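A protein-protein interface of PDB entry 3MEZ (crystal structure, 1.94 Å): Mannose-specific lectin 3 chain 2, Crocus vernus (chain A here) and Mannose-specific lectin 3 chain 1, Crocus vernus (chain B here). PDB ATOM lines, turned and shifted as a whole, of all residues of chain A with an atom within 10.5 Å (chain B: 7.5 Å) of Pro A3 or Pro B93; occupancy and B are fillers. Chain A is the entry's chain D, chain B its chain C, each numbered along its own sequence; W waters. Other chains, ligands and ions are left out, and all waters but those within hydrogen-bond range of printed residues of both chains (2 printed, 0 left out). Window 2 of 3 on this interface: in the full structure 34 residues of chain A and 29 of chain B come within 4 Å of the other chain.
Of the 11 printed residues of chain B, 4 touch a printed residue of chain A.
Printed residues of chain B that touch a printed residue of chain A: Asn B3, Tyr B19, Pro B93 and His B96.
Hydrophobic or aromatic side chains of chain B within 4 Å of the printed part of chain A: Tyr B19, Pro B93 and His B96.
Of the 21 printed residues of chain A, 7 touch a printed residue of chain B.
Along chain A the printed residues that touch a printed residue of chain B span positions 3 to 112.
Among the printed residues, no Asp or Glu carboxylate lies within 4 Å of a Lys or Arg side-chain nitrogen of the other chain.
Pro A3 touches just one residue of chain B: Pro B93 (3.9 Å).
Printed residues of chain B within 4 Å of Val A5: Asn B3 (3.9 Å), Tyr B19 (3.5 Å) and Pro B93 (3.9 Å).
Leu A21 touches none of the printed residues of chain B.
Of the printed residues of chain B, Thr A111 touches His B96.
No residue of chain A comes within 4 Å of Gly B92.
Pro B93 touches three residues of chain A.
No residue of chain A comes within 4 Å of Asp B94.
The nearest printed residue of chain B that does not touch Pro A3 is Asp B94 (6.1 Å).
ND2 of Asn B3 lies close to ND2 of Asn A7, 3.0 Å away.
Pro A3 touches Pro B93 (CG to CB, 3.9 Å).
Tyr B19 touches Arg A4 (OH to O, 3.9 Å).
CG1 of Val A5 touches ND2 of Asn B3 (3.9 Å).
Tyr B19 touches Val A5 (OH to CG2, 3.5 Å).
Val A5 touches Pro B93.
Pro B93 touches Phe A10 (CD to CZ, 3.8 Å).
CD2 of His B96 touches OG1 of Thr A111 (2.9 Å).
CD2 of His B96 touches N of Ala A112, at 3.3 Å.
N of His B96 sits at hydrogen-bond distance from OD2 of Asp B94 (3.1 Å).
N of Ala A112 sits close to OG of Ser A110, 3.2 Å away.
The backbone NH (N) of Leu B91 is in hydrogen-bond range of the backbone carbonyl oxygen (O) of Asn B3, at 3.0 Å.
The side-chain amide oxygen (OE1) of Gln A13 sits at hydrogen-bond distance from the backbone NH (N) of Phe A10, at 2.8 Å.
The backbone carbonyl oxygen (O) of Pro A3 sits at hydrogen-bond distance from the side-chain amide nitrogen (NE2) of Gln A13, at 3.0 Å.
Water W2 lies within hydrogen-bond range of the side-chain hydroxyl of Tyr B19 (2.4 Å), the backbone carbonyl oxygen of Arg A4 (2.9 Å) and the side-chain carboxylate of Glu B20 (3.4 Å).
Water W1 lies within hydrogen-bond range of OH of Tyr B19 and N of Arg A6.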
ATOM      1  N   ASN A   1      28.012 -13.568 -16.452  1.00  0.00           N
ATOM      2  CA  ASN A   1      26.665 -14.059 -16.354  1.00  0.00           C
ATOM      3  C   ASN A   1      26.072 -14.403 -17.715  1.00  0.00           C
ATOM      4  O   ASN A   1      26.070 -13.614 -18.607  1.00  0.00           O
ATOM      5  CB  ASN A   1      25.762 -13.093 -15.636  1.00  0.00           C
ATOM      6  CG  ASN A   1      26.082 -12.969 -14.181  1.00  0.00           C
ATOM      7  OD1 ASN A   1      27.197 -13.019 -13.797  1.00  0.00           O
ATOM      8  ND2 ASN A   1      25.087 -12.802 -13.400  1.00  0.00           N
ATOM      9  N   ILE A   2      25.607 -15.628 -17.813  1.00  0.00           N
ATOM     10  CA  ILE A   2      24.905 -16.122 -18.967  1.00  0.00           C
ATOM     11  C   ILE A   2      23.441 -15.616 -19.002  1.00  0.00           C
ATOM     12  O   ILE A   2      22.769 -15.703 -18.024  1.00  0.00           O
ATOM     13  CB  ILE A   2      24.930 -17.667 -18.981  1.00  0.00           C
ATOM     14  CG1 ILE A   2      26.356 -18.185 -18.862  1.00  0.00           C
ATOM     15  CG2 ILE A   2      24.264 -18.170 -20.185  1.00  0.00           C
ATOM     16  CD1 ILE A   2      26.540 -19.614 -18.478  1.00  0.00           C
ATOM     17  N   PRO A   3      22.966 -15.122 -20.135  1.00  0.00           N
ATOM     18  CA  PRO A   3      21.582 -14.700 -20.215  1.00  0.00           C
ATOM     19  C   PRO A   3      20.597 -15.844 -19.972  1.00  0.00           C
ATOM     20  O   PRO A   3      20.859 -16.929 -20.306  1.00  0.00           O
ATOM     21  CB  PRO A   3      21.459 -14.188 -21.647  1.00  0.00           C
ATOM     22  CG  PRO A   3      22.720 -13.889 -22.084  1.00  0.00           C
ATOM     23  CD  PRO A   3      23.705 -14.654 -21.306  1.00  0.00           C
ATOM     24  N   ARG A   4      19.478 -15.511 -19.372  1.00  0.00           N
ATOM     25  CA  ARG A   4      18.414 -16.432 -19.035  1.00  0.00           C
ATOM     26  C   ARG A   4      17.707 -16.929 -20.299  1.00  0.00           C
ATOM     27  O   ARG A   4      17.474 -16.193 -21.198  1.00  0.00           O
ATOM     28  CB  ARG A   4      17.465 -15.778 -18.017  1.00  0.00           C
ATOM     29  CG  ARG A   4      18.020 -15.750 -16.578  1.00  0.00           C
ATOM     30  CD  ARG A   4      17.918 -14.466 -15.706  1.00  0.00           C
ATOM     31  NE  ARG A   4      18.795 -14.630 -14.536  1.00  0.00           N
ATOM     32  CZ  ARG A   4      19.038 -13.783 -13.532  1.00  0.00           C
ATOM     33  NH1 ARG A   4      18.527 -12.554 -13.458  1.00  0.00           N
ATOM     34  NH2 ARG A   4      19.863 -14.172 -12.569  1.00  0.00           N
ATOM     35  N   VAL A   5      17.412 -18.208 -20.327  1.00  0.00           N
ATOM     36  CA  VAL A   5      16.748 -18.843 -21.440  1.00  0.00           C
ATOM     37  C   VAL A   5      15.569 -19.616 -20.894  1.00  0.00           C
ATOM     38  O   VAL A   5      15.671 -20.201 -19.875  1.00  0.00           O
ATOM     39  CB  VAL A   5      17.715 -19.753 -22.214  1.00  0.00           C
ATOM     40  CG1 VAL A   5      17.001 -20.558 -23.270  1.00  0.00           C
ATOM     41  CG2 VAL A   5      18.815 -18.929 -22.827  1.00  0.00           C
ATOM     42  N   ARG A   6      14.475 -19.611 -21.609  1.00  0.00           N
ATOM     43  CA  ARG A   6      13.218 -20.132 -21.110  1.00  0.00           C
ATOM     44  C   ARG A   6      13.168 -21.612 -20.725  1.00  0.00           C
ATOM     45  O   ARG A   6      12.564 -21.946 -19.777  1.00  0.00           O
ATOM     46  CB  ARG A   6      12.151 -19.880 -22.144  1.00  0.00           C
ATOM     47  CG  ARG A   6      10.784 -20.097 -21.696  1.00  0.00           C
ATOM     48  CD  ARG A   6       9.764 -19.533 -22.697  1.00  0.00           C
ATOM     49  NE  ARG A   6       8.449 -19.530 -22.119  1.00  0.00           N
ATOM     50  CZ  ARG A   6       7.532 -20.433 -22.375  1.00  0.00           C
ATOM     51  NH1 ARG A   6       7.797 -21.406 -23.215  1.00  0.00           N
ATOM     52  NH2 ARG A   6       6.364 -20.356 -21.783  1.00  0.00           N
ATOM     53  N   ASN A   7      13.766 -22.456 -21.539  1.00  0.00           N
ATOM     54  CA  ASN A   7      13.696 -23.899 -21.425  1.00  0.00           C
ATOM     55  C   ASN A   7      14.986 -24.633 -21.014  1.00  0.00           C
ATOM     56  O   ASN A   7      15.007 -25.811 -20.857  1.00  0.00           O
ATOM     57  CB  ASN A   7      13.146 -24.498 -22.717  1.00  0.00           C
ATOM     58  CG  ASN A   7      14.069 -24.310 -23.918  1.00  0.00           C
ATOM     59  OD1 ASN A   7      14.222 -25.189 -24.696  1.00  0.00           O
ATOM     60  ND2 ASN A   7      14.610 -23.184 -24.065  1.00  0.00           N
ATOM     61  N   VAL A   8      16.058 -23.880 -20.865  1.00  0.00           N
ATOM     62  CA  VAL A   8      17.349 -24.421 -20.546  1.00  0.00           C
ATOM     63  C   VAL A   8      18.096 -23.630 -19.445  1.00  0.00           C
ATOM     64  O   VAL A   8      18.092 -22.456 -19.475  1.00  0.00           O
ATOM     65  CB  VAL A   8      18.199 -24.444 -21.814  1.00  0.00           C
ATOM     66  CG1 VAL A   8      19.522 -24.970 -21.552  1.00  0.00           C
ATOM     67  CG2 VAL A   8      17.506 -25.198 -22.912  1.00  0.00           C
ATOM     68  N   LEU A   9      18.732 -24.318 -18.519  1.00  0.00           N
ATOM     69  CA  LEU A   9      19.597 -23.716 -17.513  1.00  0.00           C
ATOM     70  C   LEU A   9      21.033 -24.191 -17.776  1.00  0.00           C
ATOM     71  O   LEU A   9      21.224 -25.364 -17.878  1.00  0.00           O
ATOM     72  CB  LEU A   9      19.174 -24.148 -16.113  1.00  0.00           C
ATOM     73  CG  LEU A   9      19.748 -23.367 -14.932  1.00  0.00           C
ATOM     74  CD1 LEU A   9      19.058 -22.082 -14.838  1.00  0.00           C
ATOM     75  CD2 LEU A   9      19.683 -24.049 -13.611  1.00  0.00           C
ATOM     76  N   PHE A  10      21.983 -23.278 -17.890  1.00  0.00           N
ATOM     77  CA  PHE A  10      23.385 -23.580 -18.141  1.00  0.00           C
ATOM     78  C   PHE A  10      24.251 -23.613 -16.858  1.00  0.00           C
ATOM     79  O   PHE A  10      23.924 -22.999 -15.908  1.00  0.00           O
ATOM     80  CB  PHE A  10      23.995 -22.577 -19.120  1.00  0.00           C
ATOM     81  CG  PHE A  10      23.353 -22.535 -20.452  1.00  0.00           C
ATOM     82  CD1 PHE A  10      22.306 -21.711 -20.679  1.00  0.00           C
ATOM     83  CD2 PHE A  10      23.811 -23.298 -21.501  1.00  0.00           C
ATOM     84  CE1 PHE A  10      21.704 -21.654 -21.900  1.00  0.00           C
ATOM     85  CE2 PHE A  10      23.202 -23.234 -22.712  1.00  0.00           C
ATOM     86  CZ  PHE A  10      22.156 -22.418 -22.893  1.00  0.00           C
ATOM     87  N   SER A  11      25.403 -24.271 -16.883  1.00  0.00           N
ATOM     88  CA  SER A  11      26.250 -24.319 -15.688  1.00  0.00           C
ATOM     89  C   SER A  11      26.608 -22.872 -15.232  1.00  0.00           C
ATOM     90  O   SER A  11      26.823 -22.049 -16.024  1.00  0.00           O
ATOM     91  CB  SER A  11      27.506 -25.185 -15.904  1.00  0.00           C
ATOM     92  OG  SER A  11      27.249 -26.548 -16.110  1.00  0.00           O
ATOM     93  N   SER A  12      26.572 -22.649 -13.936  1.00  0.00           N
ATOM     94  CA  SER A  12      26.731 -21.396 -13.234  1.00  0.00           C
ATOM     95  C   SER A  12      25.417 -20.621 -13.032  1.00  0.00           C
ATOM     96  O   SER A  12      25.347 -19.777 -12.227  1.00  0.00           O
ATOM     97  CB  SER A  12      27.781 -20.507 -13.881  1.00  0.00           C
ATOM     98  OG  SER A  12      29.063 -20.953 -13.658  1.00  0.00           O
ATOM     99  N   GLN A  13      24.400 -20.936 -13.810  1.00  0.00           N
ATOM    100  CA  GLN A  13      23.116 -20.316 -13.669  1.00  0.00           C
ATOM    101  C   GLN A  13      22.402 -20.745 -12.410  1.00  0.00           C
ATOM    102  O   GLN A  13      22.620 -21.766 -11.916  1.00  0.00           O
ATOM    103  CB  GLN A  13      22.227 -20.479 -14.906  1.00  0.00           C
ATOM    104  CG  GLN A  13      22.702 -19.689 -16.089  1.00  0.00           C
ATOM    105  CD  GLN A  13      21.739 -19.636 -17.268  1.00  0.00           C
ATOM    106  OE1 GLN A  13      21.166 -20.582 -17.616  1.00  0.00           O
ATOM    107  NE2 GLN A  13      21.611 -18.500 -17.857  1.00  0.00           N
ATOM    108  N   VAL A  14      21.536 -19.894 -11.959  1.00  0.00           N
ATOM    109  CA  VAL A  14      20.849 -19.991 -10.724  1.00  0.00           C
ATOM    110  C   VAL A  14      19.339 -19.670 -10.884  1.00  0.00           C
ATOM    111  O   VAL A  14      18.974 -18.923 -11.711  1.00  0.00           O
ATOM    112  CB  VAL A  14      21.560 -18.984  -9.825  1.00  0.00           C
ATOM    113  CG1 VAL A  14      20.691 -17.854  -9.409  1.00  0.00           C
ATOM    114  CG2 VAL A  14      22.282 -19.621  -8.807  1.00  0.00           C
ATOM    115  N   MET A  15      18.483 -20.283 -10.088  1.00  0.00           N
ATOM    116  CA  MET A  15      17.068 -19.957 -10.039  1.00  0.00           C
ATOM    117  C   MET A  15      16.575 -19.774  -8.615  1.00  0.00           C
ATOM    118  O   MET A  15      16.962 -20.494  -7.778  1.00  0.00           O
ATOM    119  CB  MET A  15      16.216 -21.027 -10.729  1.00  0.00           C
ATOM    120  CG  MET A  15      16.698 -21.518 -12.059  1.00  0.00           C
ATOM    121  SD  MET A  15      15.654 -22.865 -12.714  1.00  0.00           S
ATOM    122  CE  MET A  15      14.399 -21.821 -13.174  1.00  0.00           C
ATOM    123  N   LEU A  21      11.848 -22.765 -15.502  1.00  0.00           N
ATOM    124  CA  LEU A  21      11.971 -23.224 -16.869  1.00  0.00           C
ATOM    125  C   LEU A  21      10.559 -23.644 -17.299  1.00  0.00           C
ATOM    126  O   LEU A  21       9.790 -24.049 -16.492  1.00  0.00           O
ATOM    127  CB  LEU A  21      12.924 -24.388 -17.000  1.00  0.00           C
ATOM    128  CG  LEU A  21      14.363 -24.322 -16.523  1.00  0.00           C
ATOM    129  CD1 LEU A  21      15.116 -25.491 -16.962  1.00  0.00           C
ATOM    130  CD2 LEU A  21      14.986 -23.094 -16.948  1.00  0.00           C
ATOM    131  N   TYR A  91      27.719 -27.892 -18.522  1.00  0.00           N
ATOM    132  CA  TYR A  91      26.548 -28.722 -18.576  1.00  0.00           C
ATOM    133  C   TYR A  91      25.293 -27.902 -18.857  1.00  0.00           C
ATOM    134  O   TYR A  91      25.276 -26.713 -18.737  1.00  0.00           O
ATOM    135  CB  TYR A  91      26.378 -29.505 -17.293  1.00  0.00           C
ATOM    136  CG  TYR A  91      27.444 -30.542 -17.026  1.00  0.00           C
ATOM    137  CD1 TYR A  91      28.733 -30.185 -16.731  1.00  0.00           C
ATOM    138  CD2 TYR A  91      27.156 -31.878 -17.091  1.00  0.00           C
ATOM    139  CE1 TYR A  91      29.694 -31.144 -16.477  1.00  0.00           C
ATOM    140  CE2 TYR A  91      28.079 -32.810 -16.869  1.00  0.00           C
ATOM    141  CZ  TYR A  91      29.364 -32.459 -16.566  1.00  0.00           C
ATOM    142  OH  TYR A  91      30.289 -33.411 -16.344  1.00  0.00           O
ATOM    143  N   VAL A  92      24.253 -28.611 -19.240  1.00  0.00           N
ATOM    144  CA  VAL A  92      22.972 -28.046 -19.425  1.00  0.00           C
ATOM    145  C   VAL A  92      21.830 -28.883 -18.769  1.00  0.00           C
ATOM    146  O   VAL A  92      21.856 -30.048 -18.769  1.00  0.00           O
ATOM    147  CB  VAL A  92      22.745 -27.796 -20.912  1.00  0.00           C
ATOM    148  CG1 VAL A  92      22.341 -28.987 -21.605  1.00  0.00           C
ATOM    149  CG2 VAL A  92      21.813 -26.742 -21.132  1.00  0.00           C
ATOM    150  N   SER A 110      31.616 -27.801 -30.007  1.00  0.00           N
ATOM    151  CA  SER A 110      30.854 -26.612 -30.308  1.00  0.00           C
ATOM    152  C   SER A 110      31.264 -25.952 -31.626  1.00  0.00           C
ATOM    153  O   SER A 110      32.357 -26.061 -32.025  1.00  0.00           O
ATOM    154  CB  SER A 110      30.968 -25.645 -29.144  1.00  0.00           C
ATOM    155  OG  SER A 110      30.498 -24.376 -29.373  1.00  0.00           O
ATOM    156  N   THR A 111      30.341 -25.253 -32.250  1.00  0.00           N
ATOM    157  CA  THR A 111      30.620 -24.431 -33.423  1.00  0.00           C
ATOM    158  C   THR A 111      31.587 -23.252 -33.122  1.00  0.00           C
ATOM    159  O   THR A 111      32.204 -22.741 -33.986  1.00  0.00           O
ATOM    160  CB  THR A 111      29.353 -23.889 -34.063  1.00  0.00           C
ATOM    161  OG1 THR A 111      28.640 -23.108 -33.122  1.00  0.00           O
ATOM    162  CG2 THR A 111      28.487 -24.997 -34.583  1.00  0.00           C
ATOM    163  N   ALA A 112      31.699 -22.858 -31.877  1.00  0.00           N
ATOM    164  CA  ALA A 112      32.575 -21.752 -31.513  1.00  0.00           C
ATOM    165  C   ALA A 112      34.006 -22.107 -31.686  1.00  0.00           C
ATOM    166  O   ALA A 112      34.403 -23.184 -31.332  1.00  0.00           O
ATOM    167  CB  ALA A 112      32.338 -21.332 -30.150  1.00  0.00           C
ATOM    168  N   ASN B   3      15.393 -24.222 -30.191  1.00  0.00           N
ATOM    169  CA  ASN B   3      16.752 -24.048 -29.772  1.00  0.00           C
ATOM    170  C   ASN B   3      17.489 -25.363 -29.382  1.00  0.00           C
ATOM    171  O   ASN B   3      18.623 -25.331 -29.059  1.00  0.00           O
ATOM    172  CB  ASN B   3      16.839 -23.027 -28.660  1.00  0.00           C
ATOM    173  CG  ASN B   3      16.169 -23.475 -27.377  1.00  0.00           C
ATOM    174  OD1 ASN B   3      15.289 -24.273 -27.370  1.00  0.00           O
ATOM    175  ND2 ASN B   3      16.626 -22.927 -26.289  1.00  0.00           N
ATOM    176  N   TYR B  19      17.663 -19.368 -32.152  1.00  0.00           N
ATOM    177  CA  TYR B  19      17.483 -18.617 -30.949  1.00  0.00           C
ATOM    178  C   TYR B  19      17.825 -17.157 -31.209  1.00  0.00           C
ATOM    179  O   TYR B  19      18.900 -16.846 -31.621  1.00  0.00           O
ATOM    180  CB  TYR B  19      18.322 -19.165 -29.809  1.00  0.00           C
ATOM    181  CG  TYR B  19      17.945 -18.584 -28.495  1.00  0.00           C
ATOM    182  CD1 TYR B  19      18.769 -17.710 -27.834  1.00  0.00           C
ATOM    183  CD2 TYR B  19      16.750 -18.880 -27.929  1.00  0.00           C
ATOM    184  CE1 TYR B  19      18.411 -17.173 -26.643  1.00  0.00           C
ATOM    185  CE2 TYR B  19      16.393 -18.354 -26.762  1.00  0.00           C
ATOM    186  CZ  TYR B  19      17.202 -17.487 -26.119  1.00  0.00           C
ATOM    187  OH  TYR B  19      16.817 -16.982 -24.952  1.00  0.00           O
ATOM    188  N   GLU B  20      16.880 -16.282 -30.956  1.00  0.00           N
ATOM    189  CA  GLU B  20      17.094 -14.857 -31.156  1.00  0.00           C
ATOM    190  C   GLU B  20      17.571 -14.606 -32.593  1.00  0.00           C
ATOM    191  O   GLU B  20      16.913 -14.970 -33.509  1.00  0.00           O
ATOM    192  CB  GLU B  20      17.962 -14.224 -30.063  1.00  0.00           C
ATOM    193  CG  GLU B  20      17.255 -14.251 -28.740  1.00  0.00           C
ATOM    194  CD  GLU B  20      18.032 -13.801 -27.536  1.00  0.00           C
ATOM    195  OE1 GLU B  20      19.226 -13.621 -27.606  1.00  0.00           O
ATOM    196  OE2 GLU B  20      17.420 -13.666 -26.491  1.00  0.00           O
ATOM    197  N   ALA B  22      20.229 -15.847 -34.127  1.00  0.00           N
ATOM    198  CA  ALA B  22      21.012 -16.933 -34.660  1.00  0.00           C
ATOM    199  C   ALA B  22      20.132 -18.053 -35.183  1.00  0.00           C
ATOM    200  O   ALA B  22      19.114 -18.311 -34.645  1.00  0.00           O
ATOM    201  CB  ALA B  22      21.937 -17.424 -33.667  1.00  0.00           C
ATOM    202  N   THR B  90      22.331 -27.636 -28.355  1.00  0.00           N
ATOM    203  CA  THR B  90      21.693 -26.405 -27.968  1.00  0.00           C
ATOM    204  C   THR B  90      22.301 -25.164 -28.672  1.00  0.00           C
ATOM    205  O   THR B  90      23.482 -24.946 -28.614  1.00  0.00           O
ATOM    206  CB  THR B  90      21.806 -26.181 -26.442  1.00  0.00           C
ATOM    207  OG1 THR B  90      21.265 -27.277 -25.737  1.00  0.00           O
ATOM    208  CG2 THR B  90      21.088 -24.954 -26.033  1.00  0.00           C
ATOM    209  N   LEU B  91      21.454 -24.367 -29.299  1.00  0.00           N
ATOM    210  CA  LEU B  91      21.832 -23.104 -29.869  1.00  0.00           C
ATOM    211  C   LEU B  91      21.611 -22.076 -28.780  1.00  0.00           C
ATOM    212  O   LEU B  91      20.516 -21.661 -28.527  1.00  0.00           O
ATOM    213  CB  LEU B  91      20.974 -22.767 -31.082  1.00  0.00           C
ATOM    214  CG  LEU B  91      21.465 -21.868 -32.218  1.00  0.00           C
ATOM    215  CD1 LEU B  91      20.362 -21.364 -33.172  1.00  0.00           C
ATOM    216  CD2 LEU B  91      22.403 -20.832 -31.782  1.00  0.00           C
ATOM    217  N   GLY B  92      22.690 -21.708 -28.123  1.00  0.00           N
ATOM    218  CA  GLY B  92      22.633 -20.873 -26.955  1.00  0.00           C
ATOM    219  C   GLY B  92      22.535 -19.390 -27.182  1.00  0.00           C
ATOM    220  O   GLY B  92      22.556 -18.952 -28.282  1.00  0.00           O
ATOM    221  N   PRO B  93      22.462 -18.650 -26.086  1.00  0.00           N
ATOM    222  CA  PRO B  93      22.465 -17.200 -26.093  1.00  0.00           C
ATOM    223  C   PRO B  93      23.766 -16.643 -26.625  1.00  0.00           C
ATOM    224  O   PRO B  93      23.834 -15.538 -27.018  1.00  0.00           O
ATOM    225  CB  PRO B  93      22.308 -16.833 -24.622  1.00  0.00           C
ATOM    226  CG  PRO B  93      22.487 -17.997 -23.906  1.00  0.00           C
ATOM    227  CD  PRO B  93      22.227 -19.143 -24.741  1.00  0.00           C
ATOM    228  N   ASP B  94      24.774 -17.479 -26.652  1.00  0.00           N
ATOM    229  CA  ASP B  94      26.065 -17.190 -27.226  1.00  0.00           C
ATOM    230  C   ASP B  94      26.113 -17.193 -28.773  1.00  0.00           C
ATOM    231  O   ASP B  94      27.111 -16.949 -29.349  1.00  0.00           O
ATOM    232  CB  ASP B  94      27.127 -18.080 -26.608  1.00  0.00           C
ATOM    233  CG  ASP B  94      26.959 -19.546 -26.964  1.00  0.00           C
ATOM    234  OD1 ASP B  94      27.843 -20.321 -26.587  1.00  0.00           O
ATOM    235  OD2 ASP B  94      25.978 -19.885 -27.626  1.00  0.00           O
ATOM    236  N   GLN B  95      25.006 -17.529 -29.398  1.00  0.00           N
ATOM    237  CA  GLN B  95      24.918 -17.646 -30.838  1.00  0.00           C
ATOM    238  C   GLN B  95      25.685 -18.827 -31.509  1.00  0.00           C
ATOM    239  O   GLN B  95      25.943 -18.824 -32.689  1.00  0.00           O
ATOM    240  CB  GLN B  95      25.251 -16.334 -31.514  1.00  0.00           C
ATOM    241  CG  GLN B  95      24.330 -15.234 -31.172  1.00  0.00           C
ATOM    242  CD  GLN B  95      24.594 -13.971 -31.936  1.00  0.00           C
ATOM    243  OE1 GLN B  95      24.732 -13.978 -33.109  1.00  0.00           O
ATOM    244  NE2 GLN B  95      24.671 -12.898 -31.244  1.00  0.00           N
ATOM    245  N   HIS B  96      25.984 -19.822 -30.710  1.00  0.00           N
ATOM    246  CA  HIS B  96      26.650 -21.013 -31.161  1.00  0.00           C
ATOM    247  C   HIS B  96      25.902 -22.286 -30.774  1.00  0.00           C
ATOM    248  O   HIS B  96      25.108 -22.284 -29.888  1.00  0.00           O
ATOM    249  CB  HIS B  96      28.060 -21.061 -30.638  1.00  0.00           C
ATOM    250  CG  HIS B  96      29.007 -20.237 -31.434  1.00  0.00           C
ATOM    251  ND1 HIS B  96      29.409 -19.000 -31.025  1.00  0.00           N
ATOM    252  CD2 HIS B  96      29.598 -20.447 -32.627  1.00  0.00           C
ATOM    253  CE1 HIS B  96      30.204 -18.478 -31.925  1.00  0.00           C
ATOM    254  NE2 HIS B  96      30.336 -19.334 -32.905  1.00  0.00           N
HETATM  255  O   HOH W   1      14.378 -17.624 -23.767  1.00  0.00           O
HETATM  256  O   HOH W   2      18.419 -15.553 -23.814  1.00  0.00           O
